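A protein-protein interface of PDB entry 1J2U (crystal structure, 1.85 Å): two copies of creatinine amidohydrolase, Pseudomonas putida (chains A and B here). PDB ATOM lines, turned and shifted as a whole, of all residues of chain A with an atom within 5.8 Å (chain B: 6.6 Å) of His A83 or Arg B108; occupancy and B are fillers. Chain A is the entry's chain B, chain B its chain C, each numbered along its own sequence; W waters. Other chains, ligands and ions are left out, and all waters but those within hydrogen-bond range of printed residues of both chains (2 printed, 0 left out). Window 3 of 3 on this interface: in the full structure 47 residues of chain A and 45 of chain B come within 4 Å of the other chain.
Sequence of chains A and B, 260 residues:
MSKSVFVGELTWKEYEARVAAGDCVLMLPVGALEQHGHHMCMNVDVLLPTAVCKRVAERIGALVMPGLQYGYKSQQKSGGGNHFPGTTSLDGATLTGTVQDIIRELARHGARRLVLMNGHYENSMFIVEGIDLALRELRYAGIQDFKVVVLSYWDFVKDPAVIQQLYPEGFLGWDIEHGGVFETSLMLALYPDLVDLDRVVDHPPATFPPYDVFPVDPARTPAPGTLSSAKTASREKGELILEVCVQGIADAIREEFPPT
OD1 of Asn A82 sits close to OE1 of Glu B105 (2.9 Å).
The guanidinium group (NH1) of Arg B108 lies close to the backbone carbonyl oxygen (O) of Asn A82 (3.0 Å).
NH1 of Arg B108 sits at hydrogen-bond distance from O of His A83 (3.4 Å).
NH1 of Arg B108 sits at hydrogen-bond distance from O of Phe A84, 2.9 Å away.
The backbone NH (N) of Gly A86 is in hydrogen-bond range of a ring nitrogen (NE2) of His B109, 3.4 Å away.
O of Thr A87 sits at hydrogen-bond distance from NH2 of Arg B108, 2.8 Å away.
A ring nitrogen (NE2) of His B109 sits at hydrogen-bond distance from the backbone carbonyl oxygen (O) of Thr A87, 2.8 Å away.
The side-chain carboxylate (OE1) of Glu B105 lies within hydrogen-bond range of the backbone NH (N) of Ser A89 (2.9 Å).
ND2 of Asn A82 is in hydrogen-bond range of OG of Ser A89.
The backbone carbonyl oxygen (O) of Gly A86 lies within hydrogen-bond range of the side-chain hydroxyl (OG1) of Thr A88, 2.8 Å away.
NE of Arg B108 is in salt-bridge range of OE2 of Glu B105, 2.9 Å away.
O of Glu B105 sits close to NE2 of His B109 (3.4 Å).
NH2 of Arg B108 lies within hydrogen-bond range of NE2 of His B109 (3.4 Å).
CA of Pro A85 touches CD2 of His B109 (3.99 Å).
O of Thr A87 touches OE1 of Glu B105, 3.5 Å away.
OE1 of Glu B105 touches CA of Thr A88 (3.7 Å).
CE1 of His B109 touches OG1 of Thr A88, 3.3 Å away.
Of chain B, only Arg B108 comes within 4 Å of His A83.
Of chain A, only Asn A82, His A83, Phe A84 and Thr A87 come within 4 Å of Arg B108.
Of the printed residues of chain B, Thr A88 touches Glu B105 (3.7 Å) and His B109 (3.3 Å).
Of the printed residues of chain A, Glu B105 touches Asn A82, Thr A87, Thr A88 and Ser A89.
Printed residues of chain B within 4 Å of Asn A82: Glu B105 (2.9 Å) and Arg B108 (2.9 Å).
Printed residues of chain B within 4 Å of Phe A84: Arg B108.
Of the printed residues of chain B, Thr A87 touches Glu B105 (3.5 Å), Arg B108 (2.8 Å) and His B109 (2.8 Å).
Leu B106 touches none of the printed residues of chain A.
Arg B112 touches none of the printed residues of chain A.
The nearest residue of chain A that does not touch Arg B108 is Pro A85 (4.5 Å).
Of the 15 printed residues of chain A, 8 touch a printed residue of chain B.
Along chain A the printed residues that touch a printed residue of chain B span positions 82 to 89.
Among the printed residues, 12 pairs touch across the chains.
No position is printed for both chains.
Of the 12 pairs that touch across the chains among the printed residues, none has its exchanged pair printed and touching as well.
Water W1 lies within hydrogen-bond range of the backbone carbonyl oxygen (O) of His A83 (2.7 Å) and the guanidinium group (NH1) of Arg B108 (3.0 Å).
Water W2 lies within hydrogen-bond range of the backbone carbonyl oxygen of Ser A89 (2.8 Å) and the guanidinium group of Arg B104 (3.3 Å).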
ATOM      1  N   GLN A  76      22.140 -21.558 -16.341  1.00  0.00           N
ATOM      2  CA  GLN A  76      23.491 -21.937 -16.770  1.00  0.00           C
ATOM      3  C   GLN A  76      24.310 -22.581 -15.662  1.00  0.00           C
ATOM      4  O   GLN A  76      24.765 -23.717 -15.799  1.00  0.00           O
ATOM      5  CB  GLN A  76      24.218 -20.709 -17.334  1.00  0.00           C
ATOM      6  CG  GLN A  76      25.616 -21.002 -17.867  1.00  0.00           C
ATOM      7  CD  GLN A  76      26.027 -19.982 -18.899  1.00  0.00           C
ATOM      8  OE1 GLN A  76      26.172 -18.803 -18.583  1.00  0.00           O
ATOM      9  NE2 GLN A  76      26.140 -20.418 -20.156  1.00  0.00           N
ATOM     10  N   GLY A  80      23.056 -25.953 -16.945  1.00  0.00           N
ATOM     11  CA  GLY A  80      23.577 -25.698 -18.280  1.00  0.00           C
ATOM     12  C   GLY A  80      22.938 -24.570 -19.073  1.00  0.00           C
ATOM     13  O   GLY A  80      23.597 -23.940 -19.893  1.00  0.00           O
ATOM     14  N   GLY A  81      21.652 -24.304 -18.850  1.00  0.00           N
ATOM     15  CA  GLY A  81      21.001 -23.201 -19.525  1.00  0.00           C
ATOM     16  C   GLY A  81      19.778 -23.632 -20.307  1.00  0.00           C
ATOM     17  O   GLY A  81      19.727 -24.745 -20.830  1.00  0.00           O
ATOM     18  N   ASN A  82      18.805 -22.738 -20.423  1.00  0.00           N
ATOM     19  CA  ASN A  82      17.558 -23.088 -21.096  1.00  0.00           C
ATOM     20  C   ASN A  82      17.608 -23.016 -22.623  1.00  0.00           C
ATOM     21  O   ASN A  82      16.584 -23.198 -23.268  1.00  0.00           O
ATOM     22  CB  ASN A  82      16.393 -22.236 -20.585  1.00  0.00           C
ATOM     23  CG  ASN A  82      15.075 -23.013 -20.599  1.00  0.00           C
ATOM     24  OD1 ASN A  82      14.174 -22.731 -21.381  1.00  0.00           O
ATOM     25  ND2 ASN A  82      14.985 -24.004 -19.754  1.00  0.00           N
ATOM     26  N   HIS A  83      18.793 -22.785 -23.190  1.00  0.00           N
ATOM     27  CA  HIS A  83      18.969 -22.722 -24.642  1.00  0.00           C
ATOM     28  C   HIS A  83      19.133 -24.104 -25.276  1.00  0.00           C
ATOM     29  O   HIS A  83      19.029 -24.240 -26.496  1.00  0.00           O
ATOM     30  CB  HIS A  83      20.183 -21.859 -25.009  1.00  0.00           C
ATOM     31  CG  HIS A  83      21.472 -22.372 -24.448  1.00  0.00           C
ATOM     32  ND1 HIS A  83      21.780 -22.297 -23.107  1.00  0.00           N
ATOM     33  CD2 HIS A  83      22.513 -23.010 -25.038  1.00  0.00           C
ATOM     34  CE1 HIS A  83      22.970 -22.832 -22.900  1.00  0.00           C
ATOM     35  NE2 HIS A  83      23.435 -23.276 -24.056  1.00  0.00           N
ATOM     36  N   PHE A  84      19.387 -25.120 -24.471  1.00  0.00           N
ATOM     37  CA  PHE A  84      19.526 -26.470 -24.997  1.00  0.00           C
ATOM     38  C   PHE A  84      18.222 -26.998 -25.551  1.00  0.00           C
ATOM     39  O   PHE A  84      17.146 -26.667 -25.046  1.00  0.00           O
ATOM     40  CB  PHE A  84      19.988 -27.452 -23.923  1.00  0.00           C
ATOM     41  CG  PHE A  84      21.456 -27.413 -23.679  1.00  0.00           C
ATOM     42  CD1 PHE A  84      22.009 -26.429 -22.877  1.00  0.00           C
ATOM     43  CD2 PHE A  84      22.296 -28.327 -24.291  1.00  0.00           C
ATOM     44  CE1 PHE A  84      23.381 -26.369 -22.670  1.00  0.00           C
ATOM     45  CE2 PHE A  84      23.672 -28.268 -24.084  1.00  0.00           C
ATOM     46  CZ  PHE A  84      24.209 -27.281 -23.285  1.00  0.00           C
ATOM     47  N   PRO A  85      18.336 -27.857 -26.559  1.00  0.00           N
ATOM     48  CA  PRO A  85      17.190 -28.596 -27.082  1.00  0.00           C
ATOM     49  C   PRO A  85      16.732 -29.613 -26.050  1.00  0.00           C
ATOM     50  O   PRO A  85      17.515 -30.007 -25.190  1.00  0.00           O
ATOM     51  CB  PRO A  85      17.773 -29.344 -28.297  1.00  0.00           C
ATOM     52  CG  PRO A  85      19.103 -28.755 -28.544  1.00  0.00           C
ATOM     53  CD  PRO A  85      19.595 -28.201 -27.254  1.00  0.00           C
ATOM     54  N   GLY A  86      15.477 -30.040 -26.121  1.00  0.00           N
ATOM     55  CA  GLY A  86      14.988 -31.051 -25.215  1.00  0.00           C
ATOM     56  C   GLY A  86      14.459 -30.482 -23.910  1.00  0.00           C
ATOM     57  O   GLY A  86      13.332 -30.779 -23.521  1.00  0.00           O
ATOM     58  N   THR A  87      15.267 -29.672 -23.239  1.00  0.00           N
ATOM     59  CA  THR A  87      14.827 -29.005 -22.010  1.00  0.00           C
ATOM     60  C   THR A  87      13.521 -28.272 -22.296  1.00  0.00           C
ATOM     61  O   THR A  87      13.467 -27.465 -23.191  1.00  0.00           O
ATOM     62  CB  THR A  87      15.885 -28.007 -21.564  1.00  0.00           C
ATOM     63  OG1 THR A  87      17.103 -28.703 -21.254  1.00  0.00           O
ATOM     64  CG2 THR A  87      15.451 -27.317 -20.276  1.00  0.00           C
ATOM     65  N   THR A  88      12.473 -28.563 -21.528  1.00  0.00           N
ATOM     66  CA  THR A  88      11.160 -27.977 -21.757  1.00  0.00           C
ATOM     67  C   THR A  88      10.682 -27.434 -20.434  1.00  0.00           C
ATOM     68  O   THR A  88      10.269 -28.200 -19.568  1.00  0.00           O
ATOM     69  CB  THR A  88      10.227 -29.070 -22.238  1.00  0.00           C
ATOM     70  OG1 THR A  88      10.763 -29.663 -23.433  1.00  0.00           O
ATOM     71  CG2 THR A  88       8.861 -28.473 -22.618  1.00  0.00           C
ATOM     72  N   SER A  89      10.735 -26.122 -20.297  1.00  0.00           N
ATOM     73  CA  SER A  89      10.546 -25.485 -19.004  1.00  0.00           C
ATOM     74  C   SER A  89       9.298 -24.629 -18.889  1.00  0.00           C
ATOM     75  O   SER A  89       8.872 -23.989 -19.849  1.00  0.00           O
ATOM     76  CB  SER A  89      11.758 -24.607 -18.736  1.00  0.00           C
ATOM     77  OG  SER A  89      12.964 -25.361 -18.797  1.00  0.00           O
ATOM     78  N   VAL A 216      21.541 -15.885 -22.195  1.00  0.00           N
ATOM     79  CA  VAL A 216      22.559 -16.846 -21.831  1.00  0.00           C
ATOM     80  C   VAL A 216      23.481 -17.078 -23.004  1.00  0.00           C
ATOM     81  O   VAL A 216      23.020 -17.247 -24.154  1.00  0.00           O
ATOM     82  CB  VAL A 216      21.964 -18.193 -21.362  1.00  0.00           C
ATOM     83  CG1 VAL A 216      20.907 -18.713 -22.344  1.00  0.00           C
ATOM     84  CG2 VAL A 216      23.086 -19.205 -21.159  1.00  0.00           C
ATOM     85  N   ASP A 217      24.773 -17.056 -22.689  1.00  0.00           N
ATOM     86  CA  ASP A 217      25.838 -17.301 -23.644  1.00  0.00           C
ATOM     87  C   ASP A 217      26.264 -18.776 -23.615  1.00  0.00           C
ATOM     88  O   ASP A 217      26.922 -19.231 -22.673  1.00  0.00           O
ATOM     89  CB  ASP A 217      27.026 -16.429 -23.295  1.00  0.00           C
ATOM     90  CG  ASP A 217      28.185 -16.647 -24.221  1.00  0.00           C
ATOM     91  OD1 ASP A 217      29.240 -16.023 -23.998  1.00  0.00           O
ATOM     92  OD2 ASP A 217      28.121 -17.431 -25.192  1.00  0.00           O
ATOM     93  N   PRO A 218      25.910 -19.515 -24.658  1.00  0.00           N
ATOM     94  CA  PRO A 218      26.174 -20.957 -24.699  1.00  0.00           C
ATOM     95  C   PRO A 218      27.642 -21.322 -24.543  1.00  0.00           C
ATOM     96  O   PRO A 218      27.934 -22.411 -24.041  1.00  0.00           O
ATOM     97  CB  PRO A 218      25.668 -21.384 -26.077  1.00  0.00           C
ATOM     98  CG  PRO A 218      25.436 -20.161 -26.840  1.00  0.00           C
ATOM     99  CD  PRO A 218      25.244 -19.033 -25.877  1.00  0.00           C
ATOM    100  N   THR A 221      28.907 -22.706 -21.132  1.00  0.00           N
ATOM    101  CA  THR A 221      28.552 -24.023 -20.610  1.00  0.00           C
ATOM    102  C   THR A 221      29.352 -25.066 -21.371  1.00  0.00           C
ATOM    103  O   THR A 221      29.466 -24.964 -22.577  1.00  0.00           O
ATOM    104  CB  THR A 221      27.068 -24.358 -20.882  1.00  0.00           C
ATOM    105  OG1 THR A 221      26.209 -23.432 -20.218  1.00  0.00           O
ATOM    106  CG2 THR A 221      26.691 -25.702 -20.284  1.00  0.00           C
ATOM    107  N   ILE B 103       4.294 -25.517 -25.550  1.00  0.00           N
ATOM    108  CA  ILE B 103       4.342 -25.141 -26.964  1.00  0.00           C
ATOM    109  C   ILE B 103       5.441 -24.128 -27.276  1.00  0.00           C
ATOM    110  O   ILE B 103       6.187 -24.283 -28.265  1.00  0.00           O
ATOM    111  CB  ILE B 103       2.964 -24.663 -27.464  1.00  0.00           C
ATOM    112  CG1 ILE B 103       1.978 -25.816 -27.433  1.00  0.00           C
ATOM    113  CG2 ILE B 103       3.091 -24.130 -28.887  1.00  0.00           C
ATOM    114  CD1 ILE B 103       0.551 -25.390 -27.682  1.00  0.00           C
ATOM    115  N   ARG B 104       5.550 -23.081 -26.461  1.00  0.00           N
ATOM    116  CA  ARG B 104       6.617 -22.108 -26.615  1.00  0.00           C
ATOM    117  C   ARG B 104       7.986 -22.806 -26.625  1.00  0.00           C
ATOM    118  O   ARG B 104       8.840 -22.527 -27.485  1.00  0.00           O
ATOM    119  CB  ARG B 104       6.561 -21.080 -25.476  1.00  0.00           C
ATOM    120  CG  ARG B 104       7.667 -20.047 -25.481  1.00  0.00           C
ATOM    121  CD  ARG B 104       7.721 -19.238 -24.193  1.00  0.00           C
ATOM    122  NE  ARG B 104       6.424 -18.640 -23.950  1.00  0.00           N
ATOM    123  CZ  ARG B 104       5.652 -18.874 -22.897  1.00  0.00           C
ATOM    124  NH1 ARG B 104       4.476 -18.277 -22.832  1.00  0.00           N
ATOM    125  NH2 ARG B 104       6.048 -19.671 -21.912  1.00  0.00           N
ATOM    126  N   GLU B 105       8.190 -23.736 -25.705  1.00  0.00           N
ATOM    127  CA  GLU B 105       9.476 -24.429 -25.625  1.00  0.00           C
ATOM    128  C   GLU B 105       9.743 -25.379 -26.816  1.00  0.00           C
ATOM    129  O   GLU B 105      10.865 -25.414 -27.358  1.00  0.00           O
ATOM    130  CB  GLU B 105       9.576 -25.165 -24.300  1.00  0.00           C
ATOM    131  CG  GLU B 105       9.741 -24.214 -23.130  1.00  0.00           C
ATOM    132  CD  GLU B 105      11.188 -23.763 -22.988  1.00  0.00           C
ATOM    133  OE1 GLU B 105      11.940 -24.436 -22.260  1.00  0.00           O
ATOM    134  OE2 GLU B 105      11.569 -22.742 -23.601  1.00  0.00           O
ATOM    135  N   LEU B 106       8.729 -26.133 -27.222  1.00  0.00           N
ATOM    136  CA  LEU B 106       8.861 -27.022 -28.371  1.00  0.00           C
ATOM    137  C   LEU B 106       9.207 -26.197 -29.616  1.00  0.00           C
ATOM    138  O   LEU B 106      10.072 -26.601 -30.422  1.00  0.00           O
ATOM    139  CB  LEU B 106       7.595 -27.855 -28.568  1.00  0.00           C
ATOM    140  CG  LEU B 106       7.313 -28.893 -27.478  1.00  0.00           C
ATOM    141  CD1 LEU B 106       6.017 -29.615 -27.741  1.00  0.00           C
ATOM    142  CD2 LEU B 106       8.456 -29.894 -27.378  1.00  0.00           C
ATOM    143  N   ALA B 107       8.586 -25.024 -29.748  1.00  0.00           N
ATOM    144  CA  ALA B 107       8.848 -24.144 -30.869  1.00  0.00           C
ATOM    145  C   ALA B 107      10.294 -23.685 -30.832  1.00  0.00           C
ATOM    146  O   ALA B 107      10.943 -23.596 -31.879  1.00  0.00           O
ATOM    147  CB  ALA B 107       7.919 -22.964 -30.872  1.00  0.00           C
ATOM    148  N   ARG B 108      10.800 -23.400 -29.628  1.00  0.00           N
ATOM    149  CA  ARG B 108      12.187 -22.992 -29.455  1.00  0.00           C
ATOM    150  C   ARG B 108      13.141 -24.086 -29.946  1.00  0.00           C
ATOM    151  O   ARG B 108      14.185 -23.783 -30.556  1.00  0.00           O
ATOM    152  CB  ARG B 108      12.467 -22.625 -27.986  1.00  0.00           C
ATOM    153  CG  ARG B 108      13.944 -22.291 -27.684  1.00  0.00           C
ATOM    154  CD  ARG B 108      14.208 -21.908 -26.215  1.00  0.00           C
ATOM    155  NE  ARG B 108      13.894 -22.975 -25.266  1.00  0.00           N
ATOM    156  CZ  ARG B 108      14.581 -24.112 -25.131  1.00  0.00           C
ATOM    157  NH1 ARG B 108      15.637 -24.363 -25.890  1.00  0.00           N
ATOM    158  NH2 ARG B 108      14.225 -24.999 -24.215  1.00  0.00           N
ATOM    159  N   HIS B 109      12.798 -25.335 -29.667  1.00  0.00           N
ATOM    160  CA  HIS B 109      13.581 -26.485 -30.119  1.00  0.00           C
ATOM    161  C   HIS B 109      13.628 -26.616 -31.637  1.00  0.00           C
ATOM    162  O   HIS B 109      14.518 -27.277 -32.171  1.00  0.00           O
ATOM    163  CB  HIS B 109      12.993 -27.792 -29.623  1.00  0.00           C
ATOM    164  CG  HIS B 109      12.891 -27.902 -28.134  1.00  0.00           C
ATOM    165  ND1 HIS B 109      12.096 -28.842 -27.528  1.00  0.00           N
ATOM    166  CD2 HIS B 109      13.461 -27.183 -27.134  1.00  0.00           C
ATOM    167  CE1 HIS B 109      12.189 -28.713 -26.213  1.00  0.00           C
ATOM    168  NE2 HIS B 109      13.004 -27.709 -25.948  1.00  0.00           N
ATOM    169  N   GLY B 110      12.638 -26.052 -32.313  1.00  0.00           N
ATOM    170  CA  GLY B 110      12.562 -26.152 -33.759  1.00  0.00           C
ATOM    171  C   GLY B 110      11.448 -27.077 -34.162  1.00  0.00           C
ATOM    172  O   GLY B 110      11.201 -27.276 -35.353  1.00  0.00           O
ATOM    173  N   ALA B 111      10.762 -27.657 -33.176  1.00  0.00           N
ATOM    174  CA  ALA B 111       9.625 -28.509 -33.462  1.00  0.00           C
ATOM    175  C   ALA B 111       8.509 -27.665 -34.044  1.00  0.00           C
ATOM    176  O   ALA B 111       8.353 -26.490 -33.695  1.00  0.00           O
ATOM    177  CB  ALA B 111       9.151 -29.222 -32.209  1.00  0.00           C
ATOM    178  N   ARG B 112       7.737 -28.259 -34.951  1.00  0.00           N
ATOM    179  CA  ARG B 112       6.627 -27.552 -35.578  1.00  0.00           C
ATOM    180  C   ARG B 112       5.358 -28.394 -35.702  1.00  0.00           C
ATOM    181  O   ARG B 112       4.355 -27.930 -36.238  1.00  0.00           O
ATOM    182  CB  ARG B 112       7.056 -27.031 -36.965  1.00  0.00           C
ATOM    183  CG  ARG B 112       8.120 -25.963 -36.923  1.00  0.00           C
ATOM    184  CD  ARG B 112       7.613 -24.667 -36.327  1.00  0.00           C
ATOM    185  NE  ARG B 112       8.535 -23.541 -36.370  1.00  0.00           N
ATOM    186  CZ  ARG B 112       9.408 -23.221 -35.425  1.00  0.00           C
ATOM    187  NH1 ARG B 112       9.566 -23.983 -34.342  1.00  0.00           N
ATOM    188  NH2 ARG B 112      10.175 -22.156 -35.593  1.00  0.00           N
ATOM    189  N   LEU B 138       3.783 -17.000 -30.892  1.00  0.00           N
ATOM    190  CA  LEU B 138       4.655 -17.401 -31.986  1.00  0.00           C
ATOM    191  C   LEU B 138       4.508 -16.412 -33.135  1.00  0.00           C
ATOM    192  O   LEU B 138       5.488 -16.011 -33.754  1.00  0.00           O
ATOM    193  CB  LEU B 138       4.362 -18.825 -32.431  1.00  0.00           C
ATOM    194  CG  LEU B 138       4.768 -19.897 -31.418  1.00  0.00           C
ATOM    195  CD1 LEU B 138       4.277 -21.250 -31.878  1.00  0.00           C
ATOM    196  CD2 LEU B 138       6.272 -19.918 -31.237  1.00  0.00           C
ATOM    197  N   ILE B 143       6.765 -16.603 -36.305  1.00  0.00           N
ATOM    198  CA  ILE B 143       6.544 -18.023 -36.558  1.00  0.00           C
ATOM    199  C   ILE B 143       5.075 -18.335 -36.839  1.00  0.00           C
ATOM    200  O   ILE B 143       4.209 -18.155 -35.975  1.00  0.00           O
ATOM    201  CB  ILE B 143       7.066 -18.814 -35.365  1.00  0.00           C
ATOM    202  CG1 ILE B 143       8.570 -18.541 -35.185  1.00  0.00           C
ATOM    203  CG2 ILE B 143       6.783 -20.302 -35.535  1.00  0.00           C
ATOM    204  CD1 ILE B 143       9.146 -19.056 -33.908  1.00  0.00           C
ATOM    205  N   PHE B 146       3.933 -23.425 -36.992  1.00  0.00           N
ATOM    206  CA  PHE B 146       3.733 -24.400 -35.934  1.00  0.00           C
ATOM    207  C   PHE B 146       2.283 -24.860 -36.062  1.00  0.00           C
ATOM    208  O   PHE B 146       1.378 -24.025 -36.116  1.00  0.00           O
ATOM    209  CB  PHE B 146       4.008 -23.779 -34.546  1.00  0.00           C
ATOM    210  CG  PHE B 146       4.218 -24.800 -33.467  1.00  0.00           C
ATOM    211  CD1 PHE B 146       3.157 -25.502 -32.955  1.00  0.00           C
ATOM    212  CD2 PHE B 146       5.487 -25.089 -32.990  1.00  0.00           C
ATOM    213  CE1 PHE B 146       3.348 -26.473 -31.981  1.00  0.00           C
ATOM    214  CE2 PHE B 146       5.677 -26.060 -32.003  1.00  0.00           C
ATOM    215  CZ  PHE B 146       4.608 -26.743 -31.503  1.00  0.00           C
HETATM  216  O   HOH W   1      17.214 -22.739 -27.840  1.00  0.00           O
HETATM  217  O   HOH W   2       8.490 -21.211 -20.312  1.00  0.00           O
